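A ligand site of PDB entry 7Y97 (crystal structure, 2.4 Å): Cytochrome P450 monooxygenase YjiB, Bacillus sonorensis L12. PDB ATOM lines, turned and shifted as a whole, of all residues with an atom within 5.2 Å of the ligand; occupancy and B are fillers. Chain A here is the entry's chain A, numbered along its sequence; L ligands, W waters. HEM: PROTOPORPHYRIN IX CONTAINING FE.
ND2 of Asn 69 lies within hydrogen-bond range of O of Val 85.
The backbone carbonyl oxygen of Ala 242 is in hydrogen-bond range of the side-chain hydroxyl of Thr 246 (2.7 Å).
The side-chain sulfur (SG) of Cys 352 lies close to the backbone NH (N) of Gly 354, at 3.5 Å.
O of Gly 243 sits at hydrogen-bond distance from OG1 of Thr 246, 3.3 Å away.
NH1 of Arg 96 is in hydrogen-bond range of O of Phe 351 (2.7 Å).
The guanidinium group (NH2) of Arg 294 lies within hydrogen-bond range of the backbone carbonyl oxygen (O) of Ile 61, at 2.7 Å.
SG of Cys 352 lies close to N of Ala 355 (3.3 Å).
A ring nitrogen (ND1) of His 350 sits at hydrogen-bond distance from a ring nitrogen (NE2) of His 92 (3.3 Å).
Water W3 lies within hydrogen-bond range of an oxygen (O1A) of the ligand and the guanidinium group (NH2) of Arg 294.
ND2 of Asn 69 is in hydrogen-bond range of O2A of the ligand, at 3.4 Å.
The side-chain sulfur (SG) of Cys 352 binds an iron atom (FE) of the ligand (2.3 Å).
An oxygen (O2A) of the ligand lies within salt-bridge range of the guanidinium group (NH1) of Arg 294, at 2.9 Å.
The guanidinium group of Arg 96 is in salt-bridge range of an oxygen (O2D) of the ligand, at 2.9 Å.
An oxygen (O1D) of the ligand lies within hydrogen-bond range of a ring nitrogen (ND1) of His 350, at 2.8 Å.
NE2 of His 92 is in hydrogen-bond range of O2D of the ligand.
The backbone carbonyl oxygen (O) of Ala 242 sits close to a nitrogen (NC) of the ligand (3.3 Å).
Merely in contact with the ligand: Gly 243 (3.3 Å), Leu 250 (3.3 Å), Thr 246 (3.4 Å), Met 84 (3.4 Å), Phe 345 (3.4 Å), Gly 346 (3.4 Å), Pro 288 (3.5 Å), Gly 344 (3.5 Å), Val 85 (3.5 Å), Leu 239 (3.5 Å), Thr 247 (3.5 Å), Gly 354 (3.6 Å), Ile 147 (3.6 Å), Leu 317 (3.7 Å), Ile 292 (3.7 Å), Ala 358 (3.7 Å), Leu 357 (3.8 Å), Leu 238 (3.8 Å), Leu 353 (3.8 Å) and Ile 349 (3.9 Å).
Hydrophobic or aromatic side chains within 4 Å of the ligand: Met 84, Val 85, His 92, Ile 147, Leu 238, Leu 239, Ala 242, Leu 250, Pro 288, Ile 292, Leu 317, Phe 345, His 350, Leu 353, Leu 357 and Ala 358.
Within 4 Å of the ligand: Asn 69, Met 84, Val 85, His 92, Arg 96, Ile 147, Leu 238, Leu 239, Ala 242, Gly 243, Thr 246, Thr 247, Leu 250, Pro 288, Ile 292, Arg 294, Leu 317, Gly 344, Phe 345, Gly 346, Ile 349, His 350, Cys 352, Leu 353, Gly 354, Leu 357 and Ala 358.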
ATOM      1  N   ILE A  61      -3.924  -0.215  36.493  1.00  0.00           N
ATOM      2  CA  ILE A  61      -3.518  -0.752  35.192  1.00  0.00           C
ATOM      3  C   ILE A  61      -4.010  -2.162  34.938  1.00  0.00           C
ATOM      4  O   ILE A  61      -3.985  -2.615  33.782  1.00  0.00           O
ATOM      5  CB  ILE A  61      -1.980  -0.690  35.060  1.00  0.00           C
ATOM      6  CG1 ILE A  61      -1.330  -1.620  36.076  1.00  0.00           C
ATOM      7  CG2 ILE A  61      -1.493   0.730  35.256  1.00  0.00           C
ATOM      8  CD1 ILE A  61       0.183  -1.618  36.019  1.00  0.00           C
ATOM      9  N   ASN A  69      -9.159   0.755  28.670  1.00  0.00           N
ATOM     10  CA  ASN A  69      -8.111   1.193  27.712  1.00  0.00           C
ATOM     11  C   ASN A  69      -8.760   1.924  26.534  1.00  0.00           C
ATOM     12  O   ASN A  69      -8.028   2.498  25.721  1.00  0.00           O
ATOM     13  CB  ASN A  69      -7.262   0.019  27.218  1.00  0.00           C
ATOM     14  CG  ASN A  69      -6.143  -0.341  28.175  1.00  0.00           C
ATOM     15  OD1 ASN A  69      -6.396  -0.668  29.329  1.00  0.00           O
ATOM     16  ND2 ASN A  69      -4.922  -0.310  27.699  1.00  0.00           N
ATOM     17  N   MET A  84      -4.737  -2.923  19.658  1.00  0.00           N
ATOM     18  CA  MET A  84      -5.198  -3.558  20.889  1.00  0.00           C
ATOM     19  C   MET A  84      -4.909  -2.722  22.126  1.00  0.00           C
ATOM     20  O   MET A  84      -5.486  -2.991  23.184  1.00  0.00           O
ATOM     21  CB  MET A  84      -4.546  -4.914  21.031  1.00  0.00           C
ATOM     22  CG  MET A  84      -3.040  -4.813  20.939  1.00  0.00           C
ATOM     23  SD  MET A  84      -2.176  -6.379  20.925  1.00  0.00           S
ATOM     24  CE  MET A  84      -0.597  -5.772  20.389  1.00  0.00           C
ATOM     25  N   VAL A  85      -4.007  -1.735  22.029  1.00  0.00           N
ATOM     26  CA  VAL A  85      -3.680  -0.927  23.195  1.00  0.00           C
ATOM     27  C   VAL A  85      -4.886  -0.097  23.622  1.00  0.00           C
ATOM     28  O   VAL A  85      -5.048   0.200  24.816  1.00  0.00           O
ATOM     29  CB  VAL A  85      -2.460  -0.036  22.898  1.00  0.00           C
ATOM     30  CG1 VAL A  85      -2.108   0.843  24.101  1.00  0.00           C
ATOM     31  CG2 VAL A  85      -1.272  -0.866  22.485  1.00  0.00           C
ATOM     32  N   HIS A  92      -9.965  -7.081  22.483  1.00  0.00           N
ATOM     33  CA  HIS A  92      -8.550  -7.166  22.823  1.00  0.00           C
ATOM     34  C   HIS A  92      -8.108  -8.621  22.989  1.00  0.00           C
ATOM     35  O   HIS A  92      -7.019  -9.005  22.536  1.00  0.00           O
ATOM     36  CB  HIS A  92      -8.268  -6.381  24.100  1.00  0.00           C
ATOM     37  CG  HIS A  92      -6.911  -6.639  24.675  1.00  0.00           C
ATOM     38  ND1 HIS A  92      -6.687  -7.566  25.665  1.00  0.00           N
ATOM     39  CD2 HIS A  92      -5.704  -6.089  24.385  1.00  0.00           C
ATOM     40  CE1 HIS A  92      -5.404  -7.586  25.972  1.00  0.00           C
ATOM     41  NE2 HIS A  92      -4.779  -6.696  25.214  1.00  0.00           N
ATOM     42  N   ARG A  96      -4.963 -10.256  21.140  1.00  0.00           N
ATOM     43  CA  ARG A  96      -3.865 -10.606  22.030  1.00  0.00           C
ATOM     44  C   ARG A  96      -3.523 -12.093  21.931  1.00  0.00           C
ATOM     45  O   ARG A  96      -2.344 -12.466  21.918  1.00  0.00           O
ATOM     46  CB  ARG A  96      -4.212 -10.237  23.469  1.00  0.00           C
ATOM     47  CG  ARG A  96      -3.170 -10.691  24.496  1.00  0.00           C
ATOM     48  CD  ARG A  96      -2.077  -9.647  24.678  1.00  0.00           C
ATOM     49  NE  ARG A  96      -1.011 -10.099  25.571  1.00  0.00           N
ATOM     50  CZ  ARG A  96      -0.063  -9.323  26.076  1.00  0.00           C
ATOM     51  NH1 ARG A  96      -0.045  -8.030  25.793  1.00  0.00           N
ATOM     52  NH2 ARG A  96       0.858  -9.831  26.883  1.00  0.00           N
ATOM     53  N   PHE A 103       5.673 -14.094  19.888  1.00  0.00           N
ATOM     54  CA  PHE A 103       6.623 -13.711  20.924  1.00  0.00           C
ATOM     55  C   PHE A 103       6.792 -14.811  21.970  1.00  0.00           C
ATOM     56  O   PHE A 103       7.068 -14.525  23.142  1.00  0.00           O
ATOM     57  CB  PHE A 103       6.201 -12.390  21.585  1.00  0.00           C
ATOM     58  CG  PHE A 103       6.093 -11.249  20.615  1.00  0.00           C
ATOM     59  CD1 PHE A 103       4.934 -11.071  19.858  1.00  0.00           C
ATOM     60  CD2 PHE A 103       7.138 -10.355  20.442  1.00  0.00           C
ATOM     61  CE1 PHE A 103       4.825 -10.030  18.964  1.00  0.00           C
ATOM     62  CE2 PHE A 103       7.037  -9.304  19.552  1.00  0.00           C
ATOM     63  CZ  PHE A 103       5.883  -9.146  18.809  1.00  0.00           C
ATOM     64  N   ILE A 147      13.988  -4.627  15.039  1.00  0.00           N
ATOM     65  CA  ILE A 147      12.596  -4.891  14.724  1.00  0.00           C
ATOM     66  C   ILE A 147      12.384  -5.032  13.219  1.00  0.00           C
ATOM     67  O   ILE A 147      11.520  -5.815  12.790  1.00  0.00           O
ATOM     68  CB  ILE A 147      11.683  -3.810  15.330  1.00  0.00           C
ATOM     69  CG1 ILE A 147      10.233  -4.279  15.362  1.00  0.00           C
ATOM     70  CG2 ILE A 147      11.807  -2.490  14.573  1.00  0.00           C
ATOM     71  CD1 ILE A 147       9.987  -5.405  16.342  1.00  0.00           C
ATOM     72  N   PHE A 235      -0.758  -3.311  13.504  1.00  0.00           N
ATOM     73  CA  PHE A 235       0.001  -3.977  14.550  1.00  0.00           C
ATOM     74  C   PHE A 235       1.501  -3.825  14.333  1.00  0.00           C
ATOM     75  O   PHE A 235       2.264  -3.669  15.289  1.00  0.00           O
ATOM     76  CB  PHE A 235      -0.379  -5.454  14.632  1.00  0.00           C
ATOM     77  CG  PHE A 235       0.476  -6.245  15.566  1.00  0.00           C
ATOM     78  CD1 PHE A 235       0.371  -6.086  16.944  1.00  0.00           C
ATOM     79  CD2 PHE A 235       1.386  -7.166  15.087  1.00  0.00           C
ATOM     80  CE1 PHE A 235       1.171  -6.819  17.806  1.00  0.00           C
ATOM     81  CE2 PHE A 235       2.186  -7.899  15.949  1.00  0.00           C
ATOM     82  CZ  PHE A 235       2.068  -7.731  17.309  1.00  0.00           C
ATOM     83  N   LEU A 238       2.438  -0.580  15.469  1.00  0.00           N
ATOM     84  CA  LEU A 238       2.446  -0.568  16.923  1.00  0.00           C
ATOM     85  C   LEU A 238       3.751  -1.098  17.487  1.00  0.00           C
ATOM     86  O   LEU A 238       4.227  -0.614  18.518  1.00  0.00           O
ATOM     87  CB  LEU A 238       1.255  -1.359  17.461  1.00  0.00           C
ATOM     88  CG  LEU A 238       1.041  -1.305  18.971  1.00  0.00           C
ATOM     89  CD1 LEU A 238       0.720   0.111  19.406  1.00  0.00           C
ATOM     90  CD2 LEU A 238      -0.066  -2.263  19.380  1.00  0.00           C
ATOM     91  N   LEU A 239       4.344  -2.102  16.821  1.00  0.00           N
ATOM     92  CA  LEU A 239       5.610  -2.654  17.308  1.00  0.00           C
ATOM     93  C   LEU A 239       6.719  -1.608  17.240  1.00  0.00           C
ATOM     94  O   LEU A 239       7.548  -1.520  18.161  1.00  0.00           O
ATOM     95  CB  LEU A 239       5.985  -3.886  16.491  1.00  0.00           C
ATOM     96  CG  LEU A 239       5.121  -5.142  16.668  1.00  0.00           C
ATOM     97  CD1 LEU A 239       5.703  -6.296  15.880  1.00  0.00           C
ATOM     98  CD2 LEU A 239       5.001  -5.515  18.136  1.00  0.00           C
ATOM     99  N   ALA A 242       5.772   1.112  19.983  1.00  0.00           N
ATOM    100  CA  ALA A 242       5.822   0.656  21.367  1.00  0.00           C
ATOM    101  C   ALA A 242       7.188   0.099  21.749  1.00  0.00           C
ATOM    102  O   ALA A 242       7.488   0.015  22.945  1.00  0.00           O
ATOM    103  CB  ALA A 242       4.743  -0.399  21.619  1.00  0.00           C
ATOM    104  N   GLY A 243       8.004  -0.274  20.775  1.00  0.00           N
ATOM    105  CA  GLY A 243       9.237  -0.956  21.074  1.00  0.00           C
ATOM    106  C   GLY A 243      10.529  -0.192  20.844  1.00  0.00           C
ATOM    107  O   GLY A 243      11.538  -0.505  21.465  1.00  0.00           O
ATOM    108  N   THR A 246      11.198   2.962  23.695  1.00  0.00           N
ATOM    109  CA  THR A 246      11.179   2.334  25.006  1.00  0.00           C
ATOM    110  C   THR A 246      12.432   1.513  25.233  1.00  0.00           C
ATOM    111  O   THR A 246      13.097   1.624  26.273  1.00  0.00           O
ATOM    112  CB  THR A 246       9.924   1.462  25.150  1.00  0.00           C
ATOM    113  OG1 THR A 246       9.897   0.476  24.111  1.00  0.00           O
ATOM    114  CG2 THR A 246       8.668   2.313  25.080  1.00  0.00           C
ATOM    115  N   THR A 247      12.780   0.661  24.265  1.00  0.00           N
ATOM    116  CA  THR A 247      13.967  -0.182  24.402  1.00  0.00           C
ATOM    117  C   THR A 247      15.236   0.660  24.387  1.00  0.00           C
ATOM    118  O   THR A 247      16.189   0.374  25.115  1.00  0.00           O
ATOM    119  CB  THR A 247      13.998  -1.216  23.278  1.00  0.00           C
ATOM    120  OG1 THR A 247      12.751  -1.917  23.240  1.00  0.00           O
ATOM    121  CG2 THR A 247      15.128  -2.213  23.494  1.00  0.00           C
ATOM    122  N   LEU A 250      15.526   2.075  27.775  1.00  0.00           N
ATOM    123  CA  LEU A 250      15.894   1.034  28.734  1.00  0.00           C
ATOM    124  C   LEU A 250      17.392   0.764  28.707  1.00  0.00           C
ATOM    125  O   LEU A 250      18.035   0.654  29.763  1.00  0.00           O
ATOM    126  CB  LEU A 250      15.116  -0.247  28.460  1.00  0.00           C
ATOM    127  CG  LEU A 250      15.544  -1.416  29.356  1.00  0.00           C
ATOM    128  CD1 LEU A 250      15.353  -1.040  30.819  1.00  0.00           C
ATOM    129  CD2 LEU A 250      14.793  -2.695  29.029  1.00  0.00           C
ATOM    130  N   VAL A 283      14.505  -1.815  34.657  1.00  0.00           N
ATOM    131  CA  VAL A 283      13.123  -1.449  34.387  1.00  0.00           C
ATOM    132  C   VAL A 283      12.463  -0.912  35.658  1.00  0.00           C
ATOM    133  O   VAL A 283      11.639   0.006  35.597  1.00  0.00           O
ATOM    134  CB  VAL A 283      12.331  -2.629  33.805  1.00  0.00           C
ATOM    135  CG1 VAL A 283      10.903  -2.225  33.534  1.00  0.00           C
ATOM    136  CG2 VAL A 283      12.976  -3.117  32.516  1.00  0.00           C
ATOM    137  N   PRO A 288      11.581   3.197  31.571  1.00  0.00           N
ATOM    138  CA  PRO A 288      11.530   3.982  30.318  1.00  0.00           C
ATOM    139  C   PRO A 288      10.164   4.550  29.982  1.00  0.00           C
ATOM    140  O   PRO A 288      10.088   5.601  29.330  1.00  0.00           O
ATOM    141  CB  PRO A 288      12.011   2.976  29.257  1.00  0.00           C
ATOM    142  CG  PRO A 288      11.768   1.642  29.851  1.00  0.00           C
ATOM    143  CD  PRO A 288      11.913   1.781  31.334  1.00  0.00           C
ATOM    144  N   ALA A 289       9.072   3.893  30.384  1.00  0.00           N
ATOM    145  CA  ALA A 289       7.720   4.400  30.154  1.00  0.00           C
ATOM    146  C   ALA A 289       7.130   4.820  31.493  1.00  0.00           C
ATOM    147  O   ALA A 289       6.493   4.010  32.180  1.00  0.00           O
ATOM    148  CB  ALA A 289       6.847   3.348  29.478  1.00  0.00           C
ATOM    149  N   ILE A 292       1.153   5.405  32.472  1.00  0.00           N
ATOM    150  CA  ILE A 292       0.178   4.679  31.685  1.00  0.00           C
ATOM    151  C   ILE A 292      -1.183   5.283  31.970  1.00  0.00           C
ATOM    152  O   ILE A 292      -1.457   5.717  33.088  1.00  0.00           O
ATOM    153  CB  ILE A 292       0.218   3.158  32.003  1.00  0.00           C
ATOM    154  CG1 ILE A 292       1.393   2.498  31.273  1.00  0.00           C
ATOM    155  CG2 ILE A 292      -1.080   2.467  31.647  1.00  0.00           C
ATOM    156  CD1 ILE A 292       1.462   2.819  29.799  1.00  0.00           C
ATOM    157  N   VAL A 293      -2.043   5.324  30.947  1.00  0.00           N
ATOM    158  CA  VAL A 293      -3.337   5.992  31.032  1.00  0.00           C
ATOM    159  C   VAL A 293      -4.450   4.956  31.020  1.00  0.00           C
ATOM    160  O   VAL A 293      -4.398   3.961  30.290  1.00  0.00           O
ATOM    161  CB  VAL A 293      -3.506   7.012  29.882  1.00  0.00           C
ATOM    162  CG1 VAL A 293      -4.896   7.626  29.895  1.00  0.00           C
ATOM    163  CG2 VAL A 293      -2.440   8.095  29.983  1.00  0.00           C
ATOM    164  N   ARG A 294      -5.484   5.211  31.834  1.00  0.00           N
ATOM    165  CA  ARG A 294      -6.688   4.401  31.894  1.00  0.00           C
ATOM    166  C   ARG A 294      -7.877   5.343  32.040  1.00  0.00           C
ATOM    167  O   ARG A 294      -7.731   6.478  32.504  1.00  0.00           O
ATOM    168  CB  ARG A 294      -6.664   3.405  33.061  1.00  0.00           C
ATOM    169  CG  ARG A 294      -5.628   2.297  32.922  1.00  0.00           C
ATOM    170  CD  ARG A 294      -6.055   1.254  31.901  1.00  0.00           C
ATOM    171  NE  ARG A 294      -5.247   0.045  32.014  1.00  0.00           N
ATOM    172  CZ  ARG A 294      -4.096  -0.146  31.384  1.00  0.00           C
ATOM    173  NH1 ARG A 294      -3.599   0.809  30.607  1.00  0.00           N
ATOM    174  NH2 ARG A 294      -3.425  -1.280  31.541  1.00  0.00           N
ATOM    175  N   LEU A 317       3.901   4.393  36.638  1.00  0.00           N
ATOM    176  CA  LEU A 317       4.690   3.183  36.854  1.00  0.00           C
ATOM    177  C   LEU A 317       6.055   3.505  37.437  1.00  0.00           C
ATOM    178  O   LEU A 317       6.569   2.760  38.287  1.00  0.00           O
ATOM    179  CB  LEU A 317       4.855   2.425  35.536  1.00  0.00           C
ATOM    180  CG  LEU A 317       3.651   2.201  34.634  1.00  0.00           C
ATOM    181  CD1 LEU A 317       4.109   1.576  33.324  1.00  0.00           C
ATOM    182  CD2 LEU A 317       2.614   1.315  35.316  1.00  0.00           C
ATOM    183  N   ILE A 343       6.502  -3.065  37.923  1.00  0.00           N
ATOM    184  CA  ILE A 343       5.422  -3.014  36.956  1.00  0.00           C
ATOM    185  C   ILE A 343       5.770  -2.033  35.833  1.00  0.00           C
ATOM    186  O   ILE A 343       4.906  -1.344  35.297  1.00  0.00           O
ATOM    187  CB  ILE A 343       4.072  -2.651  37.612  1.00  0.00           C
ATOM    188  CG1 ILE A 343       4.172  -1.340  38.394  1.00  0.00           C
ATOM    189  CG2 ILE A 343       3.607  -3.775  38.513  1.00  0.00           C
ATOM    190  CD1 ILE A 343       2.838  -0.916  38.991  1.00  0.00           C
ATOM    191  N   GLY A 344       7.056  -1.979  35.470  1.00  0.00           N
ATOM    192  CA  GLY A 344       7.482  -1.166  34.339  1.00  0.00           C
ATOM    193  C   GLY A 344       7.020  -1.708  32.998  1.00  0.00           C
ATOM    194  O   GLY A 344       6.963  -0.954  32.023  1.00  0.00           O
ATOM    195  N   PHE A 345       6.697  -3.001  32.934  1.00  0.00           N
ATOM    196  CA  PHE A 345       6.083  -3.601  31.762  1.00  0.00           C
ATOM    197  C   PHE A 345       4.563  -3.682  31.881  1.00  0.00           C
ATOM    198  O   PHE A 345       3.917  -4.325  31.040  1.00  0.00           O
ATOM    199  CB  PHE A 345       6.643  -5.008  31.518  1.00  0.00           C
ATOM    200  CG  PHE A 345       8.016  -5.040  30.905  1.00  0.00           C
ATOM    201  CD1 PHE A 345       8.267  -4.423  29.690  1.00  0.00           C
ATOM    202  CD2 PHE A 345       9.044  -5.712  31.538  1.00  0.00           C
ATOM    203  CE1 PHE A 345       9.523  -4.459  29.130  1.00  0.00           C
ATOM    204  CE2 PHE A 345      10.309  -5.748  30.981  1.00  0.00           C
ATOM    205  CZ  PHE A 345      10.546  -5.122  29.771  1.00  0.00           C
ATOM    206  N   GLY A 346       3.991  -3.040  32.886  1.00  0.00           N
ATOM    207  CA  GLY A 346       2.568  -3.129  33.122  1.00  0.00           C
ATOM    208  C   GLY A 346       2.206  -4.339  33.962  1.00  0.00           C
ATOM    209  O   GLY A 346       3.046  -4.999  34.588  1.00  0.00           O
ATOM    210  N   ILE A 349      -3.980  -7.858  31.570  1.00  0.00           N
ATOM    211  CA  ILE A 349      -4.161  -8.379  30.228  1.00  0.00           C
ATOM    212  C   ILE A 349      -3.354  -7.600  29.190  1.00  0.00           C
ATOM    213  O   ILE A 349      -3.071  -8.134  28.107  1.00  0.00           O
ATOM    214  CB  ILE A 349      -5.657  -8.367  29.834  1.00  0.00           C
ATOM    215  CG1 ILE A 349      -6.212  -6.949  29.935  1.00  0.00           C
ATOM    216  CG2 ILE A 349      -6.449  -9.354  30.684  1.00  0.00           C
ATOM    217  CD1 ILE A 349      -7.582  -6.781  29.328  1.00  0.00           C
ATOM    218  N   HIS A 350      -2.968  -6.355  29.486  1.00  0.00           N
ATOM    219  CA  HIS A 350      -2.191  -5.549  28.568  1.00  0.00           C
ATOM    220  C   HIS A 350      -0.697  -5.580  28.860  1.00  0.00           C
ATOM    221  O   HIS A 350       0.035  -4.737  28.335  1.00  0.00           O
ATOM    222  CB  HIS A 350      -2.683  -4.097  28.589  1.00  0.00           C
ATOM    223  CG  HIS A 350      -4.023  -3.898  27.943  1.00  0.00           C
ATOM    224  ND1 HIS A 350      -4.173  -3.727  26.578  1.00  0.00           N
ATOM    225  CD2 HIS A 350      -5.262  -3.820  28.468  1.00  0.00           C
ATOM    226  CE1 HIS A 350      -5.453  -3.557  26.298  1.00  0.00           C
ATOM    227  NE2 HIS A 350      -6.142  -3.620  27.427  1.00  0.00           N
ATOM    228  N   PHE A 351      -0.252  -6.517  29.704  1.00  0.00           N
ATOM    229  CA  PHE A 351       1.165  -6.652  30.021  1.00  0.00           C
ATOM    230  C   PHE A 351       1.984  -6.652  28.732  1.00  0.00           C
ATOM    231  O   PHE A 351       1.616  -7.303  27.763  1.00  0.00           O
ATOM    232  CB  PHE A 351       1.415  -7.937  30.812  1.00  0.00           C
ATOM    233  CG  PHE A 351       2.858  -8.171  31.174  1.00  0.00           C
ATOM    234  CD1 PHE A 351       3.376  -7.646  32.340  1.00  0.00           C
ATOM    235  CD2 PHE A 351       3.683  -8.904  30.341  1.00  0.00           C
ATOM    236  CE1 PHE A 351       4.693  -7.865  32.682  1.00  0.00           C
ATOM    237  CE2 PHE A 351       5.005  -9.123  30.675  1.00  0.00           C
ATOM    238  CZ  PHE A 351       5.514  -8.598  31.836  1.00  0.00           C
ATOM    239  N   CYS A 352       3.071  -5.878  28.747  1.00  0.00           N
ATOM    240  CA  CYS A 352       3.856  -5.610  27.548  1.00  0.00           C
ATOM    241  C   CYS A 352       4.013  -6.860  26.697  1.00  0.00           C
ATOM    242  O   CYS A 352       4.590  -7.860  27.136  1.00  0.00           O
ATOM    243  CB  CYS A 352       5.227  -5.077  27.949  1.00  0.00           C
ATOM    244  SG  CYS A 352       6.287  -4.726  26.534  1.00  0.00           S
ATOM    245  N   LEU A 353       3.454  -6.817  25.480  1.00  0.00           N
ATOM    246  CA  LEU A 353       3.554  -7.959  24.580  1.00  0.00           C
ATOM    247  C   LEU A 353       4.996  -8.219  24.177  1.00  0.00           C
ATOM    248  O   LEU A 353       5.385  -9.383  24.009  1.00  0.00           O
ATOM    249  CB  LEU A 353       2.684  -7.717  23.343  1.00  0.00           C
ATOM    250  CG  LEU A 353       2.667  -8.843  22.317  1.00  0.00           C
ATOM    251  CD1 LEU A 353       1.991 -10.085  22.894  1.00  0.00           C
ATOM    252  CD2 LEU A 353       1.985  -8.374  21.048  1.00  0.00           C
ATOM    253  N   GLY A 354       5.802  -7.175  24.043  1.00  0.00           N
ATOM    254  CA  GLY A 354       7.179  -7.277  23.622  1.00  0.00           C
ATOM    255  C   GLY A 354       8.199  -7.412  24.735  1.00  0.00           C
ATOM    256  O   GLY A 354       9.399  -7.362  24.452  1.00  0.00           O
ATOM    257  N   ALA A 355       7.769  -7.596  25.982  1.00  0.00           N
ATOM    258  CA  ALA A 355       8.718  -7.754  27.082  1.00  0.00           C
ATOM    259  C   ALA A 355       9.745  -8.852  26.826  1.00  0.00           C
ATOM    260  O   ALA A 355      10.936  -8.605  27.072  1.00  0.00           O
ATOM    261  CB  ALA A 355       7.954  -8.001  28.393  1.00  0.00           C
ATOM    262  N   LEU A 357      11.076  -9.675  24.048  1.00  0.00           N
ATOM    263  CA  LEU A 357      12.043  -9.120  23.108  1.00  0.00           C
ATOM    264  C   LEU A 357      12.861  -8.000  23.735  1.00  0.00           C
ATOM    265  O   LEU A 357      14.077  -7.930  23.528  1.00  0.00           O
ATOM    266  CB  LEU A 357      11.334  -8.632  21.847  1.00  0.00           C
ATOM    267  CG  LEU A 357      12.228  -7.930  20.818  1.00  0.00           C
ATOM    268  CD1 LEU A 357      13.392  -8.832  20.435  1.00  0.00           C
ATOM    269  CD2 LEU A 357      11.428  -7.526  19.587  1.00  0.00           C
ATOM    270  N   ALA A 358      12.200  -7.110  24.476  1.00  0.00           N
ATOM    271  CA  ALA A 358      12.934  -6.053  25.182  1.00  0.00           C
ATOM    272  C   ALA A 358      13.946  -6.648  26.145  1.00  0.00           C
ATOM    273  O   ALA A 358      15.075  -6.132  26.253  1.00  0.00           O
ATOM    274  CB  ALA A 358      11.954  -5.145  25.929  1.00  0.00           C
HETATM  275  CHA HEM L   1       2.362  -2.610  26.030  1.00  0.00           C
HETATM  276  CHB HEM L   1       6.308  -1.132  28.402  1.00  0.00           C
HETATM  277  CHC HEM L   1       9.156  -2.740  24.784  1.00  0.00           C
HETATM  278  CHD HEM L   1       5.199  -3.897  22.302  1.00  0.00           C
HETATM  279  C1A HEM L   1       3.187  -2.111  27.015  1.00  0.00           C
HETATM  280  C2A HEM L   1       2.771  -1.644  28.320  1.00  0.00           C
HETATM  281  C3A HEM L   1       3.858  -1.234  28.977  1.00  0.00           C
HETATM  282  C4A HEM L   1       4.998  -1.424  28.106  1.00  0.00           C
HETATM  283  CMA HEM L   1       3.888  -0.670  30.411  1.00  0.00           C
HETATM  284  CAA HEM L   1       1.320  -1.646  28.847  1.00  0.00           C
HETATM  285  CBA HEM L   1       0.556  -0.433  28.319  1.00  0.00           C
HETATM  286  CGA HEM L   1      -0.844  -0.492  28.882  1.00  0.00           C
HETATM  287  O1A HEM L   1      -1.119  -1.418  29.684  1.00  0.00           O
HETATM  288  O2A HEM L   1      -1.672   0.377  28.526  1.00  0.00           O
HETATM  289  C1B HEM L   1       7.412  -1.454  27.632  1.00  0.00           C
HETATM  290  C2B HEM L   1       8.777  -1.221  28.022  1.00  0.00           C
HETATM  291  C3B HEM L   1       9.565  -1.654  27.021  1.00  0.00           C
HETATM  292  C4B HEM L   1       8.724  -2.183  25.981  1.00  0.00           C
HETATM  293  CMB HEM L   1       9.153  -0.562  29.367  1.00  0.00           C
HETATM  294  CAB HEM L   1      11.115  -1.661  26.893  1.00  0.00           C
HETATM  295  CBB HEM L   1      11.932  -1.403  27.913  1.00  0.00           C
HETATM  296  C1C HEM L   1       8.344  -3.228  23.794  1.00  0.00           C
HETATM  297  C2C HEM L   1       8.773  -3.895  22.569  1.00  0.00           C
HETATM  298  C3C HEM L   1       7.651  -4.217  21.885  1.00  0.00           C
HETATM  299  C4C HEM L   1       6.520  -3.766  22.655  1.00  0.00           C
HETATM  300  CMC HEM L   1      10.250  -4.154  22.206  1.00  0.00           C
HETATM  301  CAC HEM L   1       7.478  -4.927  20.520  1.00  0.00           C
HETATM  302  CBC HEM L   1       8.481  -5.163  19.656  1.00  0.00           C
HETATM  303  C1D HEM L   1       4.111  -3.655  23.111  1.00  0.00           C
HETATM  304  C2D HEM L   1       2.755  -3.888  22.726  1.00  0.00           C
HETATM  305  C3D HEM L   1       1.952  -3.545  23.740  1.00  0.00           C
HETATM  306  C4D HEM L   1       2.791  -3.067  24.810  1.00  0.00           C
HETATM  307  CMD HEM L   1       2.353  -4.458  21.359  1.00  0.00           C
HETATM  308  CAD HEM L   1       0.411  -3.618  23.792  1.00  0.00           C
HETATM  309  CBD HEM L   1      -0.015  -4.810  24.644  1.00  0.00           C
HETATM  310  CGD HEM L   1      -1.520  -4.921  24.736  1.00  0.00           C
HETATM  311  O1D HEM L   1      -2.222  -3.898  24.538  1.00  0.00           O
HETATM  312  O2D HEM L   1      -2.020  -6.034  25.025  1.00  0.00           O
HETATM  313  NA  HEM L   1       4.561  -1.955  26.913  1.00  0.00           N
HETATM  314  NB  HEM L   1       7.407  -2.048  26.390  1.00  0.00           N
HETATM  315  NC  HEM L   1       6.972  -3.173  23.812  1.00  0.00           N
HETATM  316  ND  HEM L   1       4.110  -3.141  24.393  1.00  0.00           N
HETATM  317 FE   HEM L   1       5.784  -2.749  25.463  1.00  0.00          FE
HETATM  318  O   HOH W   1      -0.928   3.234  27.677  1.00  0.00           O
HETATM  319  O   HOH W   2       5.770  -0.304  24.631  1.00  0.00           O
HETATM  320  O   HOH W   3      -0.593  -2.820  32.007  1.00  0.00           O
